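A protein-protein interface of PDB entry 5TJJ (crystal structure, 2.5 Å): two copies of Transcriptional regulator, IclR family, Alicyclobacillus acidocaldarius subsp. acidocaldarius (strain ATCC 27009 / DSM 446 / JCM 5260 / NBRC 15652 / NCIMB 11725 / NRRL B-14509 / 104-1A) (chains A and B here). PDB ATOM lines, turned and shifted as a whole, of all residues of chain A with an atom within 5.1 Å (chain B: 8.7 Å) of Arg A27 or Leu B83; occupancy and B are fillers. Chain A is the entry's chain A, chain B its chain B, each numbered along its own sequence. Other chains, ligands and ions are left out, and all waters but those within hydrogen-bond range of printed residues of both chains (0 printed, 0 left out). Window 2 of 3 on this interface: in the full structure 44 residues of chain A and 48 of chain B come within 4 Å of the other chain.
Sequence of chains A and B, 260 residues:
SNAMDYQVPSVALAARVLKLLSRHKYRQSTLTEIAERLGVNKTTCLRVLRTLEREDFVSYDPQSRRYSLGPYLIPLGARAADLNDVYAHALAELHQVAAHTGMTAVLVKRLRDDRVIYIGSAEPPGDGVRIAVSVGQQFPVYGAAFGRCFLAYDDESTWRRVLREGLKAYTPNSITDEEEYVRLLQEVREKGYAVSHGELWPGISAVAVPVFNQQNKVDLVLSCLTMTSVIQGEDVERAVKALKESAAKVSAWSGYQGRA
Among the printed residues, merely in contact across the chains: Leu A21 with Leu B83 (3.6 Å), Ser A22 with Arg B79 (3.6 Å), Ser A22 with Leu B83 (3.5 Å), His A24 with Leu B83 (3.4 Å), Arg A27 with Leu B83 (3.6 Å), Leu A69 with Leu B76 (3.7 Å), Leu A69 with Arg B79 (3.9998 Å) and Leu A69 with Ala B80 (3.7 Å).
No position is printed for both chains. Of the 8 pairs that touch across the chains among the printed residues, none has its exchanged pair printed and touching as well.
Hydrophobic or aromatic side chains of chain B within 4 Å of the printed part of chain A: Ala B80 and Leu B83. Of the 12 printed residues of chain A, 5 touch a printed residue of chain B. Among the printed residues, 8 pairs touch across the chains. Among the printed residues, no Asp or Glu carboxylate lies within 4 Å of a Lys or Arg side-chain nitrogen of the other chain.
NH1 of Arg B79 is in salt-bridge range of OD2 of Asp B82, 2.8 Å away.
Arg A27 touches one residue of chain B. Of the printed residues of chain A, Leu B83 touches Leu A21, Ser A22, His A24 and Arg A27. His A24 touches just one residue of chain B: Leu B83. Printed residues of chain A within 4 Å of Leu B76: Leu A69. Of the printed residues of chain A, Arg B79 touches Ser A22 (3.6 Å) and Leu A69 (3.9998 Å). Tyr B87 touches none of the printed residues of chain A. The nearest residue of chain A that does not touch Leu B83 is Leu A69 (4.4 Å).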
ATOM      1  N   LEU A  21     -27.755   7.905  22.155  1.00  0.00           N
ATOM      2  CA  LEU A  21     -26.354   7.859  21.712  1.00  0.00           C
ATOM      3  C   LEU A  21     -25.504   9.068  22.105  1.00  0.00           C
ATOM      4  O   LEU A  21     -24.295   9.045  21.939  1.00  0.00           O
ATOM      5  CB  LEU A  21     -26.280   7.619  20.202  1.00  0.00           C
ATOM      6  CG  LEU A  21     -26.827   6.238  19.772  1.00  0.00           C
ATOM      7  CD1 LEU A  21     -26.784   6.120  18.264  1.00  0.00           C
ATOM      8  CD2 LEU A  21     -26.055   5.088  20.426  1.00  0.00           C
ATOM      9  N   SER A  22     -26.143  10.108  22.633  1.00  0.00           N
ATOM     10  CA  SER A  22     -25.479  11.303  23.068  1.00  0.00           C
ATOM     11  C   SER A  22     -25.087  11.211  24.531  1.00  0.00           C
ATOM     12  O   SER A  22     -24.491  12.142  25.037  1.00  0.00           O
ATOM     13  CB  SER A  22     -26.397  12.529  22.841  1.00  0.00           C
ATOM     14  OG  SER A  22     -27.435  12.596  23.803  1.00  0.00           O
ATOM     15  N   ARG A  23     -25.453  10.127  25.213  1.00  0.00           N
ATOM     16  CA  ARG A  23     -25.010   9.881  26.598  1.00  0.00           C
ATOM     17  C   ARG A  23     -23.678   9.182  26.563  1.00  0.00           C
ATOM     18  O   ARG A  23     -23.540   8.175  25.867  1.00  0.00           O
ATOM     19  CB  ARG A  23     -25.983   8.975  27.353  1.00  0.00           C
ATOM     20  CG  ARG A  23     -27.427   9.435  27.360  1.00  0.00           C
ATOM     21  CD  ARG A  23     -28.294   8.463  28.143  1.00  0.00           C
ATOM     22  NE  ARG A  23     -28.418   8.878  29.541  1.00  0.00           N
ATOM     23  CZ  ARG A  23     -29.499   9.428  30.094  1.00  0.00           C
ATOM     24  NH1 ARG A  23     -30.622   9.632  29.383  1.00  0.00           N
ATOM     25  NH2 ARG A  23     -29.464   9.763  31.384  1.00  0.00           N
ATOM     26  N   HIS A  24     -22.717   9.690  27.334  1.00  0.00           N
ATOM     27  CA  HIS A  24     -21.360   9.128  27.349  1.00  0.00           C
ATOM     28  C   HIS A  24     -21.375   7.610  27.475  1.00  0.00           C
ATOM     29  O   HIS A  24     -20.631   6.937  26.777  1.00  0.00           O
ATOM     30  CB  HIS A  24     -20.450   9.728  28.469  1.00  0.00           C
ATOM     31  CG  HIS A  24     -18.994   9.712  28.106  1.00  0.00           C
ATOM     32  ND1 HIS A  24     -18.213   8.583  28.213  1.00  0.00           N
ATOM     33  CD2 HIS A  24     -18.210  10.657  27.535  1.00  0.00           C
ATOM     34  CE1 HIS A  24     -17.001   8.844  27.756  1.00  0.00           C
ATOM     35  NE2 HIS A  24     -16.978  10.093  27.331  1.00  0.00           N
ATOM     36  N   LYS A  25     -22.239   7.090  28.347  1.00  0.00           N
ATOM     37  CA  LYS A  25     -22.311   5.668  28.593  1.00  0.00           C
ATOM     38  C   LYS A  25     -22.684   4.874  27.339  1.00  0.00           C
ATOM     39  O   LYS A  25     -22.056   3.868  27.052  1.00  0.00           O
ATOM     40  CB  LYS A  25     -23.287   5.363  29.731  1.00  0.00           C
ATOM     41  CG  LYS A  25     -23.098   3.981  30.351  1.00  0.00           C
ATOM     42  CD  LYS A  25     -23.749   3.885  31.731  1.00  0.00           C
ATOM     43  CE  LYS A  25     -25.256   4.178  31.671  1.00  0.00           C
ATOM     44  NZ  LYS A  25     -25.923   4.186  33.003  1.00  0.00           N
ATOM     45  N   TYR A  26     -23.657   5.359  26.574  1.00  0.00           N
ATOM     46  CA  TYR A  26     -24.168   4.662  25.393  1.00  0.00           C
ATOM     47  C   TYR A  26     -23.595   5.186  24.076  1.00  0.00           C
ATOM     48  O   TYR A  26     -24.186   4.958  23.023  1.00  0.00           O
ATOM     49  CB  TYR A  26     -25.705   4.749  25.387  1.00  0.00           C
ATOM     50  CG  TYR A  26     -26.331   4.077  26.577  1.00  0.00           C
ATOM     51  CD1 TYR A  26     -26.617   2.710  26.567  1.00  0.00           C
ATOM     52  CD2 TYR A  26     -26.595   4.789  27.731  1.00  0.00           C
ATOM     53  CE1 TYR A  26     -27.165   2.079  27.678  1.00  0.00           C
ATOM     54  CE2 TYR A  26     -27.140   4.176  28.838  1.00  0.00           C
ATOM     55  CZ  TYR A  26     -27.427   2.826  28.809  1.00  0.00           C
ATOM     56  OH  TYR A  26     -27.982   2.250  29.939  1.00  0.00           O
ATOM     57  N   ARG A  27     -22.451   5.869  24.114  1.00  0.00           N
ATOM     58  CA  ARG A  27     -21.918   6.533  22.916  1.00  0.00           C
ATOM     59  C   ARG A  27     -21.531   5.619  21.771  1.00  0.00           C
ATOM     60  O   ARG A  27     -21.592   6.027  20.607  1.00  0.00           O
ATOM     61  CB  ARG A  27     -20.721   7.409  23.255  1.00  0.00           C
ATOM     62  CG  ARG A  27     -19.489   6.644  23.695  1.00  0.00           C
ATOM     63  CD  ARG A  27     -18.415   7.573  24.218  1.00  0.00           C
ATOM     64  NE  ARG A  27     -17.528   6.826  25.094  1.00  0.00           N
ATOM     65  CZ  ARG A  27     -16.200   6.819  25.066  1.00  0.00           C
ATOM     66  NH1 ARG A  27     -15.517   7.581  24.208  1.00  0.00           N
ATOM     67  NH2 ARG A  27     -15.556   6.047  25.940  1.00  0.00           N
ATOM     68  N   GLN A  28     -21.073   4.418  22.116  1.00  0.00           N
ATOM     69  CA  GLN A  28     -20.857   3.322  21.160  1.00  0.00           C
ATOM     70  C   GLN A  28     -21.709   2.128  21.625  1.00  0.00           C
ATOM     71  O   GLN A  28     -21.303   1.385  22.542  1.00  0.00           O
ATOM     72  CB  GLN A  28     -19.373   2.933  21.079  1.00  0.00           C
ATOM     73  CG  GLN A  28     -18.449   4.034  20.574  1.00  0.00           C
ATOM     74  CD  GLN A  28     -18.531   4.313  19.075  1.00  0.00           C
ATOM     75  OE1 GLN A  28     -19.056   3.514  18.278  1.00  0.00           O
ATOM     76  NE2 GLN A  28     -17.992   5.466  18.676  1.00  0.00           N
ATOM     77  N   SER A  29     -22.881   1.957  20.997  1.00  0.00           N
ATOM     78  CA  SER A  29     -23.887   0.985  21.467  1.00  0.00           C
ATOM     79  C   SER A  29     -24.282  -0.044  20.408  1.00  0.00           C
ATOM     80  O   SER A  29     -24.534   0.324  19.255  1.00  0.00           O
ATOM     81  CB  SER A  29     -25.121   1.741  21.943  1.00  0.00           C
ATOM     82  OG  SER A  29     -24.840   2.448  23.131  1.00  0.00           O
ATOM     83  N   TYR A  67     -23.062   1.466  17.139  1.00  0.00           N
ATOM     84  CA  TYR A  67     -23.568   2.675  16.521  1.00  0.00           C
ATOM     85  C   TYR A  67     -23.225   3.875  17.399  1.00  0.00           C
ATOM     86  O   TYR A  67     -23.102   3.763  18.629  1.00  0.00           O
ATOM     87  CB  TYR A  67     -25.100   2.601  16.345  1.00  0.00           C
ATOM     88  CG  TYR A  67     -25.592   1.495  15.421  1.00  0.00           C
ATOM     89  CD1 TYR A  67     -25.778   1.724  14.055  1.00  0.00           C
ATOM     90  CD2 TYR A  67     -25.872   0.218  15.908  1.00  0.00           C
ATOM     91  CE1 TYR A  67     -26.241   0.712  13.206  1.00  0.00           C
ATOM     92  CE2 TYR A  67     -26.315  -0.795  15.064  1.00  0.00           C
ATOM     93  CZ  TYR A  67     -26.506  -0.546  13.713  1.00  0.00           C
ATOM     94  OH  TYR A  67     -26.941  -1.564  12.875  1.00  0.00           O
ATOM     95  N   SER A  68     -23.112   5.033  16.761  1.00  0.00           N
ATOM     96  CA  SER A  68     -22.764   6.255  17.448  1.00  0.00           C
ATOM     97  C   SER A  68     -23.312   7.427  16.691  1.00  0.00           C
ATOM     98  O   SER A  68     -23.710   7.283  15.521  1.00  0.00           O
ATOM     99  CB  SER A  68     -21.250   6.389  17.541  1.00  0.00           C
ATOM    100  OG  SER A  68     -20.678   6.214  16.258  1.00  0.00           O
ATOM    101  N   LEU A  69     -23.341   8.575  17.367  1.00  0.00           N
ATOM    102  CA  LEU A  69     -23.737   9.824  16.713  1.00  0.00           C
ATOM    103  C   LEU A  69     -22.906  10.092  15.466  1.00  0.00           C
ATOM    104  O   LEU A  69     -21.689  10.103  15.528  1.00  0.00           O
ATOM    105  CB  LEU A  69     -23.618  11.007  17.662  1.00  0.00           C
ATOM    106  CG  LEU A  69     -24.618  11.030  18.826  1.00  0.00           C
ATOM    107  CD1 LEU A  69     -24.501  12.322  19.611  1.00  0.00           C
ATOM    108  CD2 LEU A  69     -26.054  10.850  18.346  1.00  0.00           C
ATOM    109  N   PRO B  75     -26.990  20.716  21.761  1.00  0.00           N
ATOM    110  CA  PRO B  75     -26.220  19.753  22.544  1.00  0.00           C
ATOM    111  C   PRO B  75     -25.988  18.455  21.816  1.00  0.00           C
ATOM    112  O   PRO B  75     -24.993  17.833  22.063  1.00  0.00           O
ATOM    113  CB  PRO B  75     -27.054  19.531  23.799  1.00  0.00           C
ATOM    114  CG  PRO B  75     -28.415  19.922  23.413  1.00  0.00           C
ATOM    115  CD  PRO B  75     -28.258  21.032  22.427  1.00  0.00           C
ATOM    116  N   LEU B  76     -26.883  18.083  20.910  1.00  0.00           N
ATOM    117  CA  LEU B  76     -26.743  16.884  20.122  1.00  0.00           C
ATOM    118  C   LEU B  76     -25.509  16.958  19.235  1.00  0.00           C
ATOM    119  O   LEU B  76     -24.694  16.019  19.201  1.00  0.00           O
ATOM    120  CB  LEU B  76     -27.990  16.698  19.291  1.00  0.00           C
ATOM    121  CG  LEU B  76     -28.134  15.404  18.520  1.00  0.00           C
ATOM    122  CD1 LEU B  76     -28.077  14.224  19.491  1.00  0.00           C
ATOM    123  CD2 LEU B  76     -29.449  15.417  17.744  1.00  0.00           C
ATOM    124  N   GLY B  77     -25.341  18.091  18.561  1.00  0.00           N
ATOM    125  CA  GLY B  77     -24.182  18.314  17.720  1.00  0.00           C
ATOM    126  C   GLY B  77     -22.897  18.483  18.505  1.00  0.00           C
ATOM    127  O   GLY B  77     -21.839  18.024  18.106  1.00  0.00           O
ATOM    128  N   ALA B  78     -22.968  19.178  19.626  1.00  0.00           N
ATOM    129  CA  ALA B  78     -21.793  19.284  20.465  1.00  0.00           C
ATOM    130  C   ALA B  78     -21.360  17.861  20.894  1.00  0.00           C
ATOM    131  O   ALA B  78     -20.187  17.551  20.799  1.00  0.00           O
ATOM    132  CB  ALA B  78     -22.055  20.187  21.655  1.00  0.00           C
ATOM    133  N   ARG B  79     -22.297  16.997  21.312  1.00  0.00           N
ATOM    134  CA  ARG B  79     -21.951  15.638  21.746  1.00  0.00           C
ATOM    135  C   ARG B  79     -21.398  14.804  20.580  1.00  0.00           C
ATOM    136  O   ARG B  79     -20.531  13.965  20.758  1.00  0.00           O
ATOM    137  CB  ARG B  79     -23.143  14.884  22.366  1.00  0.00           C
ATOM    138  CG  ARG B  79     -23.754  15.405  23.658  1.00  0.00           C
ATOM    139  CD  ARG B  79     -22.829  15.341  24.865  1.00  0.00           C
ATOM    140  NE  ARG B  79     -21.875  16.451  24.871  1.00  0.00           N
ATOM    141  CZ  ARG B  79     -22.177  17.739  25.079  1.00  0.00           C
ATOM    142  NH1 ARG B  79     -21.207  18.626  25.020  1.00  0.00           N
ATOM    143  NH2 ARG B  79     -23.420  18.149  25.366  1.00  0.00           N
ATOM    144  N   ALA B  80     -21.908  15.006  19.382  1.00  0.00           N
ATOM    145  CA  ALA B  80     -21.409  14.220  18.250  1.00  0.00           C
ATOM    146  C   ALA B  80     -19.955  14.577  17.977  1.00  0.00           C
ATOM    147  O   ALA B  80     -19.212  13.778  17.438  1.00  0.00           O
ATOM    148  CB  ALA B  80     -22.267  14.430  17.011  1.00  0.00           C
ATOM    149  N   ALA B  81     -19.569  15.793  18.352  1.00  0.00           N
ATOM    150  CA  ALA B  81     -18.184  16.215  18.272  1.00  0.00           C
ATOM    151  C   ALA B  81     -17.426  15.618  19.400  1.00  0.00           C
ATOM    152  O   ALA B  81     -16.529  14.826  19.145  1.00  0.00           O
ATOM    153  CB  ALA B  81     -18.059  17.728  18.278  1.00  0.00           C
ATOM    154  N   ASP B  82     -17.812  15.898  20.643  1.00  0.00           N
ATOM    155  CA  ASP B  82     -16.929  15.565  21.777  1.00  0.00           C
ATOM    156  C   ASP B  82     -16.958  14.112  22.308  1.00  0.00           C
ATOM    157  O   ASP B  82     -16.072  13.721  23.092  1.00  0.00           O
ATOM    158  CB  ASP B  82     -17.028  16.606  22.913  1.00  0.00           C
ATOM    159  CG  ASP B  82     -18.351  16.584  23.664  1.00  0.00           C
ATOM    160  OD1 ASP B  82     -19.018  15.534  23.755  1.00  0.00           O
ATOM    161  OD2 ASP B  82     -18.721  17.638  24.224  1.00  0.00           O
ATOM    162  N   LEU B  83     -17.941  13.314  21.913  1.00  0.00           N
ATOM    163  CA  LEU B  83     -17.966  11.892  22.308  1.00  0.00           C
ATOM    164  C   LEU B  83     -17.088  11.023  21.441  1.00  0.00           C
ATOM    165  O   LEU B  83     -16.749   9.934  21.844  1.00  0.00           O
ATOM    166  CB  LEU B  83     -19.379  11.331  22.253  1.00  0.00           C
ATOM    167  CG  LEU B  83     -20.341  11.920  23.275  1.00  0.00           C
ATOM    168  CD1 LEU B  83     -21.721  11.396  22.959  1.00  0.00           C
ATOM    169  CD2 LEU B  83     -19.925  11.556  24.694  1.00  0.00           C
ATOM    170  N   ASN B  84     -16.782  11.505  20.240  1.00  0.00           N
ATOM    171  CA  ASN B  84     -15.899  10.870  19.262  1.00  0.00           C
ATOM    172  C   ASN B  84     -14.496  11.505  19.321  1.00  0.00           C
ATOM    173  O   ASN B  84     -14.308  12.705  19.041  1.00  0.00           O
ATOM    174  CB  ASN B  84     -16.502  11.093  17.858  1.00  0.00           C
ATOM    175  CG  ASN B  84     -15.822  10.265  16.773  1.00  0.00           C
ATOM    176  OD1 ASN B  84     -14.610  10.317  16.589  1.00  0.00           O
ATOM    177  ND2 ASN B  84     -16.618   9.521  16.021  1.00  0.00           N
ATOM    178  N   ASP B  85     -13.509  10.679  19.612  1.00  0.00           N
ATOM    179  CA  ASP B  85     -12.127  11.118  19.677  1.00  0.00           C
ATOM    180  C   ASP B  85     -11.615  11.753  18.382  1.00  0.00           C
ATOM    181  O   ASP B  85     -10.882  12.721  18.428  1.00  0.00           O
ATOM    182  CB  ASP B  85     -11.216   9.941  20.089  1.00  0.00           C
ATOM    183  CG  ASP B  85     -11.319   9.604  21.573  1.00  0.00           C
ATOM    184  OD1 ASP B  85     -11.672  10.492  22.376  1.00  0.00           O
ATOM    185  OD2 ASP B  85     -11.020   8.455  21.953  1.00  0.00           O
ATOM    186  N   VAL B  86     -12.022  11.229  17.236  1.00  0.00           N
ATOM    187  CA  VAL B  86     -11.542  11.755  15.974  1.00  0.00           C
ATOM    188  C   VAL B  86     -12.065  13.168  15.722  1.00  0.00           C
ATOM    189  O   VAL B  86     -11.278  14.069  15.389  1.00  0.00           O
ATOM    190  CB  VAL B  86     -11.870  10.821  14.797  1.00  0.00           C
ATOM    191  CG1 VAL B  86     -11.411  11.438  13.487  1.00  0.00           C
ATOM    192  CG2 VAL B  86     -11.165   9.500  14.993  1.00  0.00           C
ATOM    193  N   TYR B  87     -13.373  13.372  15.900  1.00  0.00           N
ATOM    194  CA  TYR B  87     -13.962  14.668  15.614  1.00  0.00           C
ATOM    195  C   TYR B  87     -13.555  15.701  16.680  1.00  0.00           C
ATOM    196  O   TYR B  87     -13.238  16.819  16.350  1.00  0.00           O
ATOM    197  CB  TYR B  87     -15.489  14.568  15.395  1.00  0.00           C
ATOM    198  CG  TYR B  87     -15.898  13.632  14.252  1.00  0.00           C
ATOM    199  CD1 TYR B  87     -15.491  13.862  12.949  1.00  0.00           C
ATOM    200  CD2 TYR B  87     -16.710  12.537  14.477  1.00  0.00           C
ATOM    201  CE1 TYR B  87     -15.860  13.009  11.909  1.00  0.00           C
ATOM    202  CE2 TYR B  87     -17.084  11.675  13.455  1.00  0.00           C
ATOM    203  CZ  TYR B  87     -16.652  11.910  12.170  1.00  0.00           C
ATOM    204  OH  TYR B  87     -17.036  11.055  11.154  1.00  0.00           O
ATOM    205  N   ALA B  88     -13.511  15.319  17.949  1.00  0.00           N
ATOM    206  CA  ALA B  88     -13.126  16.260  19.023  1.00  0.00           C
ATOM    207  C   ALA B  88     -11.756  16.860  18.778  1.00  0.00           C
ATOM    208  O   ALA B  88     -11.588  18.058  18.904  1.00  0.00           O
ATOM    209  CB  ALA B  88     -13.156  15.582  20.390  1.00  0.00           C
ATOM    210  N   HIS B  89     -10.788  16.024  18.409  1.00  0.00           N
ATOM    211  CA  HIS B  89      -9.411  16.480  18.192  1.00  0.00           C
ATOM    212  C   HIS B  89      -9.241  17.250  16.888  1.00  0.00           C
ATOM    213  O   HIS B  89      -8.487  18.222  16.848  1.00  0.00           O
ATOM    214  CB  HIS B  89      -8.416  15.323  18.283  1.00  0.00           C
ATOM    215  CG  HIS B  89      -8.217  14.835  19.680  1.00  0.00           C
ATOM    216  ND1 HIS B  89      -9.018  13.870  20.256  1.00  0.00           N
ATOM    217  CD2 HIS B  89      -7.347  15.221  20.639  1.00  0.00           C
ATOM    218  CE1 HIS B  89      -8.634  13.667  21.501  1.00  0.00           C
ATOM    219  NE2 HIS B  89      -7.618  14.468  21.758  1.00  0.00           N
